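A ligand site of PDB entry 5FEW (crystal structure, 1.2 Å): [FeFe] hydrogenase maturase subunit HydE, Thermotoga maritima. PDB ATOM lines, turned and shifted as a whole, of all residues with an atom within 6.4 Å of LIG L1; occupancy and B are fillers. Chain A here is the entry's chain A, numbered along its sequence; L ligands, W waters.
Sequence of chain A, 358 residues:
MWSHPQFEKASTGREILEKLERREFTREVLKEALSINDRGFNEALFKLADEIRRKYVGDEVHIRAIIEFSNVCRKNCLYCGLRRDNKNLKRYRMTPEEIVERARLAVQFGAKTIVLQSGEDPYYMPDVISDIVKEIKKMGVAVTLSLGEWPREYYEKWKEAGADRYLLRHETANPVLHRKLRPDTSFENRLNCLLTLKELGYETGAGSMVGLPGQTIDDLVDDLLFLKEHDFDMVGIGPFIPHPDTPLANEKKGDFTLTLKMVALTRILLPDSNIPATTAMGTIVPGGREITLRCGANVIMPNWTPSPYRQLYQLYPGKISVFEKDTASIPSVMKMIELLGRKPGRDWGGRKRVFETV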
ATOM      1  N   CYS A  73     -18.930  20.502  26.378  1.00  0.00           N
ATOM      2  CA  CYS A  73     -20.071  21.369  26.150  1.00  0.00           C
ATOM      3  C   CYS A  73     -21.362  20.712  26.603  1.00  0.00           C
ATOM      4  O   CYS A  73     -21.606  19.543  26.399  1.00  0.00           O
ATOM      5  CB  CYS A  73     -20.221  21.744  24.656  1.00  0.00           C
ATOM      6  SG  CYS A  73     -21.349  23.185  24.490  1.00  0.00           S
ATOM      7  N   CYS A  77     -25.773  21.857  19.731  1.00  0.00           N
ATOM      8  CA  CYS A  77     -25.945  22.522  18.453  1.00  0.00           C
ATOM      9  C   CYS A  77     -25.740  21.552  17.315  1.00  0.00           C
ATOM     10  O   CYS A  77     -24.782  20.778  17.311  1.00  0.00           O
ATOM     11  CB  CYS A  77     -25.000  23.756  18.305  1.00  0.00           C
ATOM     12  SG  CYS A  77     -25.140  24.919  19.678  1.00  0.00           S
ATOM     13  N   TYR A  79     -24.791  21.646  14.261  1.00  0.00           N
ATOM     14  CA  TYR A  79     -23.659  21.826  13.331  1.00  0.00           C
ATOM     15  C   TYR A  79     -22.318  21.477  13.944  1.00  0.00           C
ATOM     16  O   TYR A  79     -21.302  21.325  13.212  1.00  0.00           O
ATOM     17  CB  TYR A  79     -23.585  23.219  12.801  1.00  0.00           C
ATOM     18  CG  TYR A  79     -23.829  24.310  13.804  1.00  0.00           C
ATOM     19  CD1 TYR A  79     -22.805  24.766  14.663  1.00  0.00           C
ATOM     20  CD2 TYR A  79     -25.058  24.923  13.991  1.00  0.00           C
ATOM     21  CE1 TYR A  79     -23.029  25.732  15.592  1.00  0.00           C
ATOM     22  CE2 TYR A  79     -25.282  25.874  14.961  1.00  0.00           C
ATOM     23  CZ  TYR A  79     -24.259  26.286  15.763  1.00  0.00           C
ATOM     24  OH  TYR A  79     -24.507  27.253  16.716  1.00  0.00           O
ATOM     25  N   CYS A  80     -22.222  21.415  15.299  1.00  0.00           N
ATOM     26  CA  CYS A  80     -20.956  21.548  15.994  1.00  0.00           C
ATOM     27  C   CYS A  80     -20.388  20.182  16.419  1.00  0.00           C
ATOM     28  O   CYS A  80     -21.077  19.396  17.128  1.00  0.00           O
ATOM     29  CB  CYS A  80     -21.130  22.410  17.217  1.00  0.00           C
ATOM     30  SG  CYS A  80     -19.578  22.699  18.100  1.00  0.00           S
ATOM     31  N   LEU A  82     -18.462  19.616  18.835  1.00  0.00           N
ATOM     32  CA  LEU A  82     -18.349  19.541  20.274  1.00  0.00           C
ATOM     33  C   LEU A  82     -19.706  19.277  20.951  1.00  0.00           C
ATOM     34  O   LEU A  82     -19.777  19.163  22.146  1.00  0.00           O
ATOM     35  CB  LEU A  82     -17.742  20.811  20.911  1.00  0.00           C
ATOM     36  CG  LEU A  82     -16.378  21.183  20.369  1.00  0.00           C
ATOM     37  CD1 LEU A  82     -15.845  22.351  21.231  1.00  0.00           C
ATOM     38  CD2 LEU A  82     -15.399  20.173  20.088  1.00  0.00           C
ATOM     39  N   GLN A 117     -11.489  30.581  24.642  1.00  0.00           N
ATOM     40  CA  GLN A 117     -12.669  29.995  24.042  1.00  0.00           C
ATOM     41  C   GLN A 117     -12.834  28.617  24.561  1.00  0.00           C
ATOM     42  O   GLN A 117     -11.881  27.861  24.750  1.00  0.00           O
ATOM     43  CB  GLN A 117     -12.627  30.023  22.523  1.00  0.00           C
ATOM     44  CG  GLN A 117     -13.967  29.630  21.853  1.00  0.00           C
ATOM     45  CD  GLN A 117     -13.954  29.665  20.412  1.00  0.00           C
ATOM     46  OE1 GLN A 117     -13.473  28.676  19.796  1.00  0.00           O
ATOM     47  NE2 GLN A 117     -14.430  30.680  19.794  1.00  0.00           N
ATOM     48  N   SER A 118     -14.114  28.193  24.695  1.00  0.00           N
ATOM     49  CA  SER A 118     -14.401  26.830  25.106  1.00  0.00           C
ATOM     50  C   SER A 118     -15.782  26.448  24.624  1.00  0.00           C
ATOM     51  O   SER A 118     -16.608  27.291  24.257  1.00  0.00           O
ATOM     52  CB  SER A 118     -14.325  26.721  26.632  1.00  0.00           C
ATOM     53  OG  SER A 118     -15.246  27.550  27.299  1.00  0.00           O
ATOM     54  N   GLY A 119     -16.064  25.135  24.741  1.00  0.00           N
ATOM     55  CA  GLY A 119     -17.460  24.709  24.831  1.00  0.00           C
ATOM     56  C   GLY A 119     -18.121  25.360  26.034  1.00  0.00           C
ATOM     57  O   GLY A 119     -17.435  25.909  26.932  1.00  0.00           O
ATOM     58  N   GLU A 120     -19.449  25.270  26.141  1.00  0.00           N
ATOM     59  CA  GLU A 120     -20.127  25.704  27.341  1.00  0.00           C
ATOM     60  C   GLU A 120     -19.908  24.668  28.440  1.00  0.00           C
ATOM     61  O   GLU A 120     -20.746  23.782  28.686  1.00  0.00           O
ATOM     62  CB  GLU A 120     -21.616  25.956  27.125  1.00  0.00           C
ATOM     63  CG  GLU A 120     -21.889  27.154  26.230  1.00  0.00           C
ATOM     64  CD  GLU A 120     -23.319  27.612  26.265  1.00  0.00           C
ATOM     65  OE1 GLU A 120     -24.110  27.075  27.084  1.00  0.00           O
ATOM     66  OE2 GLU A 120     -23.689  28.520  25.478  1.00  0.00           O
ATOM     67  N   SER A 146     -14.894  33.909  24.930  1.00  0.00           N
ATOM     68  CA  SER A 146     -15.842  33.343  23.963  1.00  0.00           C
ATOM     69  C   SER A 146     -16.310  31.998  24.560  1.00  0.00           C
ATOM     70  O   SER A 146     -15.835  30.951  24.220  1.00  0.00           O
ATOM     71  CB  SER A 146     -15.180  33.137  22.639  1.00  0.00           C
ATOM     72  OG  SER A 146     -16.028  32.665  21.639  1.00  0.00           O
ATOM     73  N   LEU A 147     -17.256  32.127  25.521  1.00  0.00           N
ATOM     74  CA  LEU A 147     -17.634  31.023  26.416  1.00  0.00           C
ATOM     75  C   LEU A 147     -19.088  30.631  26.214  1.00  0.00           C
ATOM     76  O   LEU A 147     -19.563  29.723  26.898  1.00  0.00           O
ATOM     77  CB  LEU A 147     -17.356  31.330  27.863  1.00  0.00           C
ATOM     78  CG  LEU A 147     -16.002  31.897  28.155  1.00  0.00           C
ATOM     79  CD1 LEU A 147     -15.836  32.208  29.644  1.00  0.00           C
ATOM     80  CD2 LEU A 147     -14.873  31.004  27.702  1.00  0.00           C
ATOM     81  N   GLY A 148     -19.818  31.287  25.316  1.00  0.00           N
ATOM     82  CA  GLY A 148     -21.237  30.952  25.116  1.00  0.00           C
ATOM     83  C   GLY A 148     -22.159  31.804  25.963  1.00  0.00           C
ATOM     84  O   GLY A 148     -21.848  32.917  26.401  1.00  0.00           O
ATOM     85  N   GLU A 149     -23.361  31.224  26.156  1.00  0.00           N
ATOM     86  CA  GLU A 149     -24.458  31.885  26.856  1.00  0.00           C
ATOM     87  C   GLU A 149     -24.484  31.533  28.343  1.00  0.00           C
ATOM     88  O   GLU A 149     -24.554  30.369  28.681  1.00  0.00           O
ATOM     89  CB  GLU A 149     -25.777  31.384  26.259  1.00  0.00           C
ATOM     90  CG  GLU A 149     -25.946  31.728  24.804  1.00  0.00           C
ATOM     91  CD  GLU A 149     -27.090  31.080  24.052  1.00  0.00           C
ATOM     92  OE1 GLU A 149     -28.161  30.886  24.714  1.00  0.00           O
ATOM     93  OE2 GLU A 149     -26.962  30.729  22.882  1.00  0.00           O
ATOM     94  N   LEU A 167     -16.900  37.492  22.468  1.00  0.00           N
ATOM     95  CA  LEU A 167     -17.345  37.022  21.162  1.00  0.00           C
ATOM     96  C   LEU A 167     -18.507  36.078  21.342  1.00  0.00           C
ATOM     97  O   LEU A 167     -18.334  35.058  21.990  1.00  0.00           O
ATOM     98  CB  LEU A 167     -16.219  36.295  20.437  1.00  0.00           C
ATOM     99  CG  LEU A 167     -14.934  36.984  20.316  1.00  0.00           C
ATOM    100  CD1 LEU A 167     -13.892  36.083  19.651  1.00  0.00           C
ATOM    101  CD2 LEU A 167     -15.064  38.303  19.662  1.00  0.00           C
ATOM    102  N   LEU A 168     -19.636  36.388  20.741  1.00  0.00           N
ATOM    103  CA  LEU A 168     -20.816  35.526  20.826  1.00  0.00           C
ATOM    104  C   LEU A 168     -21.519  35.629  19.460  1.00  0.00           C
ATOM    105  O   LEU A 168     -22.406  36.457  19.263  1.00  0.00           O
ATOM    106  CB  LEU A 168     -21.705  35.964  21.976  1.00  0.00           C
ATOM    107  CG  LEU A 168     -22.819  34.998  22.297  1.00  0.00           C
ATOM    108  CD1 LEU A 168     -22.321  33.738  22.945  1.00  0.00           C
ATOM    109  CD2 LEU A 168     -23.827  35.666  23.276  1.00  0.00           C
ATOM    110  N   ARG A 169     -21.040  34.820  18.531  1.00  0.00           N
ATOM    111  CA  ARG A 169     -21.646  34.880  17.200  1.00  0.00           C
ATOM    112  C   ARG A 169     -23.137  34.715  17.292  1.00  0.00           C
ATOM    113  O   ARG A 169     -23.597  33.833  18.039  1.00  0.00           O
ATOM    114  CB  ARG A 169     -21.092  33.843  16.288  1.00  0.00           C
ATOM    115  CG  ARG A 169     -19.683  34.125  15.944  1.00  0.00           C
ATOM    116  CD  ARG A 169     -19.406  33.196  14.812  1.00  0.00           C
ATOM    117  NE  ARG A 169     -18.065  33.240  14.446  1.00  0.00           N
ATOM    118  CZ  ARG A 169     -17.568  32.556  13.375  1.00  0.00           C
ATOM    119  NH1 ARG A 169     -18.382  31.700  12.686  1.00  0.00           N
ATOM    120  NH2 ARG A 169     -16.354  32.772  13.047  1.00  0.00           N
ATOM    121  N   GLU A 171     -24.956  33.530  14.918  1.00  0.00           N
ATOM    122  CA  GLU A 171     -25.070  32.300  14.172  1.00  0.00           C
ATOM    123  C   GLU A 171     -26.022  32.398  12.932  1.00  0.00           C
ATOM    124  O   GLU A 171     -25.604  32.145  11.799  1.00  0.00           O
ATOM    125  CB  GLU A 171     -25.478  31.111  15.090  1.00  0.00           C
ATOM    126  CG  GLU A 171     -24.617  30.936  16.354  1.00  0.00           C
ATOM    127  CD  GLU A 171     -23.156  30.715  16.121  1.00  0.00           C
ATOM    128  OE1 GLU A 171     -22.669  30.730  14.949  1.00  0.00           O
ATOM    129  OE2 GLU A 171     -22.455  30.510  17.157  1.00  0.00           O
ATOM    130  N   ARG A 182     -30.111  25.053  17.155  1.00  0.00           N
ATOM    131  CA  ARG A 182     -29.556  25.275  18.474  1.00  0.00           C
ATOM    132  C   ARG A 182     -30.717  24.975  19.477  1.00  0.00           C
ATOM    133  O   ARG A 182     -31.293  25.898  20.089  1.00  0.00           O
ATOM    134  CB  ARG A 182     -29.013  26.681  18.612  1.00  0.00           C
ATOM    135  CG  ARG A 182     -28.026  27.009  17.521  1.00  0.00           C
ATOM    136  CD  ARG A 182     -27.300  28.315  17.693  1.00  0.00           C
ATOM    137  NE  ARG A 182     -26.379  28.188  18.827  1.00  0.00           N
ATOM    138  CZ  ARG A 182     -26.516  28.751  20.016  1.00  0.00           C
ATOM    139  NH1 ARG A 182     -27.372  29.703  20.258  1.00  0.00           N
ATOM    140  NH2 ARG A 182     -25.709  28.354  21.026  1.00  0.00           N
ATOM    141  N   ARG A 190     -29.976  34.503  22.588  1.00  0.00           N
ATOM    142  CA  ARG A 190     -28.664  34.908  22.058  1.00  0.00           C
ATOM    143  C   ARG A 190     -28.532  36.413  21.971  1.00  0.00           C
ATOM    144  O   ARG A 190     -27.532  37.006  22.371  1.00  0.00           O
ATOM    145  CB  ARG A 190     -28.474  34.235  20.672  1.00  0.00           C
ATOM    146  CG  ARG A 190     -27.058  34.223  20.137  1.00  0.00           C
ATOM    147  CD  ARG A 190     -26.295  33.170  20.793  1.00  0.00           C
ATOM    148  NE  ARG A 190     -24.987  32.835  20.159  1.00  0.00           N
ATOM    149  CZ  ARG A 190     -24.088  31.964  20.635  1.00  0.00           C
ATOM    150  NH1 ARG A 190     -24.398  31.268  21.702  1.00  0.00           N
ATOM    151  NH2 ARG A 190     -22.925  31.834  20.035  1.00  0.00           N
ATOM    152  N   TYR A 313     -10.105  19.849  19.530  1.00  0.00           N
ATOM    153  CA  TYR A 313     -11.037  20.949  19.493  1.00  0.00           C
ATOM    154  C   TYR A 313     -11.464  21.108  18.052  1.00  0.00           C
ATOM    155  O   TYR A 313     -10.977  21.992  17.357  1.00  0.00           O
ATOM    156  CB  TYR A 313     -10.437  22.208  20.057  1.00  0.00           C
ATOM    157  CG  TYR A 313     -11.477  23.269  20.397  1.00  0.00           C
ATOM    158  CD1 TYR A 313     -12.053  23.335  21.681  1.00  0.00           C
ATOM    159  CD2 TYR A 313     -11.866  24.205  19.508  1.00  0.00           C
ATOM    160  CE1 TYR A 313     -12.932  24.325  22.063  1.00  0.00           C
ATOM    161  CE2 TYR A 313     -12.713  25.230  19.847  1.00  0.00           C
ATOM    162  CZ  TYR A 313     -13.246  25.287  21.110  1.00  0.00           C
ATOM    163  OH  TYR A 313     -13.991  26.355  21.486  1.00  0.00           O
ATOM    164  N   LEU A 315     -14.456  21.711  15.926  1.00  0.00           N
ATOM    165  CA  LEU A 315     -15.821  22.125  15.641  1.00  0.00           C
ATOM    166  C   LEU A 315     -16.294  21.614  14.324  1.00  0.00           C
ATOM    167  O   LEU A 315     -17.448  21.291  14.162  1.00  0.00           O
ATOM    168  CB  LEU A 315     -15.932  23.706  15.650  1.00  0.00           C
ATOM    169  CG  LEU A 315     -15.340  24.454  16.850  1.00  0.00           C
ATOM    170  CD1 LEU A 315     -15.387  25.922  16.573  1.00  0.00           C
ATOM    171  CD2 LEU A 315     -15.902  24.066  18.022  1.00  0.00           C
HETATM  172  N1  LIG L   1     -19.463  27.618  22.692  1.00  0.00           N
HETATM  173  C1  LIG L   1     -19.263  29.042  22.404  1.00  0.00           C
HETATM  174  C2  LIG L   1     -20.337  29.482  21.475  1.00  0.00           C
HETATM  175  O1  LIG L   1     -20.493  30.738  21.325  1.00  0.00           O
HETATM  176  C3  LIG L   1     -17.815  29.383  21.792  1.00  0.00           C
HETATM  177  C4  LIG L   1     -17.719  29.060  20.275  1.00  0.00           C
HETATM  178  S1  LIG L   1     -18.192  27.414  19.712  1.00  0.00           S
HETATM  179  C5  LIG L   1     -16.786  26.519  20.434  1.00  0.00           C
HETATM  180  O2  LIG L   1     -21.013  28.593  20.879  1.00  0.00           O
HETATM  181 FE1  LG2 L   2     -20.504  23.898  19.815  1.00  0.00          FE
HETATM  182 FE2  LG2 L   2     -21.301  23.954  22.368  1.00  0.00          FE
HETATM  183 FE3  LG2 L   2     -22.917  24.940  20.421  1.00  0.00          FE
HETATM  184 FE4  LG2 L   2     -20.483  26.467  21.059  1.00  0.00          FE
HETATM  185  S1  LG2 L   2     -22.467  25.966  22.392  1.00  0.00           S
HETATM  186  S2  LG2 L   2     -21.387  25.845  18.950  1.00  0.00           S
HETATM  187  S3  LG2 L   2     -19.230  24.479  21.553  1.00  0.00           S
HETATM  188  S4  LG2 L   2     -22.285  22.738  20.741  1.00  0.00           S
HETATM  189  N1  LG3 L   3     -18.681  24.831  10.667  1.00  0.00           N
HETATM  190  C1  LG3 L   3     -19.079  24.974  12.972  1.00  0.00           C
HETATM  191  C2  LG3 L   3     -19.299  25.809  14.884  1.00  0.00           C
HETATM  192  C3  LG3 L   3     -18.192  26.100  10.755  1.00  0.00           C
HETATM  193  C4  LG3 L   3     -19.041  24.238  11.789  1.00  0.00           C
HETATM  194  N2  LG3 L   3     -18.217  26.884  11.835  1.00  0.00           N
HETATM  195  C5  LG3 L   3     -18.667  26.268  12.898  1.00  0.00           C
HETATM  196  O1  LG3 L   3     -12.574  28.194  13.448  1.00  0.00           O
HETATM  197  C6  LG3 L   3     -12.998  29.377  13.257  1.00  0.00           C
HETATM  198  O2  LG3 L   3     -13.235  29.790  12.143  1.00  0.00           O
HETATM  199  C7  LG3 L   3     -13.345  30.105  14.506  1.00  0.00           C
HETATM  200  N3  LG3 L   3     -13.187  31.572  14.167  1.00  0.00           N
HETATM  201  C8  LG3 L   3     -14.639  29.653  15.081  1.00  0.00           C
HETATM  202  S1  LG3 L   3     -15.273  30.720  16.388  1.00  0.00           S
HETATM  203  C9  LG3 L   3     -16.757  29.815  16.981  1.00  0.00           C
HETATM  204  C10 LG3 L   3     -17.855  29.735  15.921  1.00  0.00           C
HETATM  205  O3  LG3 L   3     -17.524  28.571  15.024  1.00  0.00           O
HETATM  206  C11 LG3 L   3     -19.239  29.295  16.386  1.00  0.00           C
HETATM  207  O4  LG3 L   3     -19.897  30.478  16.989  1.00  0.00           O
HETATM  208  C12 LG3 L   3     -19.943  28.845  15.104  1.00  0.00           C
HETATM  209  O5  LG3 L   3     -20.310  29.981  14.304  1.00  0.00           O
HETATM  210  C13 LG3 L   3     -18.686  28.251  14.334  1.00  0.00           C
HETATM  211  N4  LG3 L   3     -18.792  26.792  14.116  1.00  0.00           N
HETATM  212  N5  LG3 L   3     -19.438  24.628  14.251  1.00  0.00           N
HETATM  213  N6  LG3 L   3     -19.485  22.949  11.706  1.00  0.00           N
HETATM  214  O   HOH W   1     -18.968  32.540  22.793  1.00  0.00           O
HETATM  215  O   HOH W   2     -23.284  28.447  18.803  1.00  0.00           O
HETATM  216  O   HOH W   3     -23.159  29.112  22.930  1.00  0.00           O
HETATM  217  O   HOH W   4     -19.591  32.257  19.136  1.00  0.00           O
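O1 of LIG L1 lies within salt-bridge range of NH2 of Arg 190 (3.0 Å). The backbone carbonyl oxygen (O) of Ser 118 sits close to a nitrogen (N1) of LIG L1 (3.3 Å). An iron atom (FE2) of LG2 L2 is bound by the side-chain sulfur (SG) of Cys 73, 2.3 Å away. The side-chain sulfur (SG) of Cys 80 is bound to an iron atom (FE1) of LG2 L2 (2.3 Å). N of Cys 77 sits close to S4 of LG2 L2. An iron atom (FE3) of LG2 L2 is bound by the side-chain sulfur of Cys 77, at 2.3 Å. NE2 of Gln 117 sits close to S1 of LG3 L3 (3.5 Å). The side-chain carboxylate (OE1) of Glu 171 lies within hydrogen-bond range of an oxygen (O5) of LG3 L3, at 2.6 Å. O5 of LG3 L3 sits at hydrogen-bond distance from NH1 of Arg 169, at 3.0 Å. A nitrogen (N6) of LG3 L3 lies within hydrogen-bond range of the backbone carbonyl oxygen (O) of Tyr 79, at 2.9 Å.
An oxygen (O2) of LIG L1 is bound to an iron atom (FE4) of LG2 L2, 2.2 Å away.
The guanidinium group (NH2) of Arg 190 is in salt-bridge range of the side-chain carboxylate (OE2) of Glu 171 (3.2 Å). O of Arg 169 is in hydrogen-bond range of NE of Arg 190, at 2.7 Å. The side-chain carboxylate (OE2) of Glu 149 is in salt-bridge range of the guanidinium group (NH1) of Arg 190, 2.9 Å away. The side-chain hydroxyl (OH) of Tyr 313 sits at hydrogen-bond distance from the side-chain amide oxygen (OE1) of Gln 117 (2.9 Å). The backbone NH of Ser 118 lies within hydrogen-bond range of the backbone carbonyl oxygen of Ser 146 (3.3 Å). OG of Ser 146 sits at hydrogen-bond distance from NE2 of Gln 117, 3.1 Å away. The side-chain hydroxyl of Ser 146 lies within hydrogen-bond range of the backbone carbonyl oxygen of Leu 167 (3.3 Å).
Residues that only touch LIG L1: Tyr 313 (3.0 Å), Ser 146 (3.5 Å), Leu 315 (3.6 Å), Gln 117 (3.7 Å), Gly 148 (3.7 Å) and Leu 168 (3.9 Å). Hydrophobic or aromatic side chains that line LIG L1: Leu 168, Tyr 313 and Leu 315. Of the 21 residues printed, 8 come within 4 Å of LIG L1. The nearest printed residue that does not touch LIG L1 is Gly 119 (4.1 Å).
Water W1 lies within hydrogen-bond range of O of Leu 167 (2.7 Å), O1 of LIG L1 (2.8 Å), N of Gly 148 (2.9 Å), OG of Ser 146 (3.2 Å) and N of Leu 147 (3.2 Å). Water W4 lies within hydrogen-bond range of an oxygen (O4) of LG3 L3 (2.8 Å), an oxygen (O1) of LIG L1 (2.8 Å), the backbone NH of Arg 169 (3.0 Å) and the guanidinium group of Arg 190 (3.5 Å). Water W3 lies within hydrogen-bond range of the side-chain carboxylate (OE2) of Glu 120 (2.7 Å), the guanidinium group (NH1) of Arg 190 (2.8 Å), a sulfur (S1) of LG2 L2 (3.3 Å) and the guanidinium group (NH2) of Arg 182 (3.3 Å). Water W2 lies within hydrogen-bond range of OH of Tyr 79, OE2 of Glu 171, NE of Arg 182 and S2 of LG2 L2.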
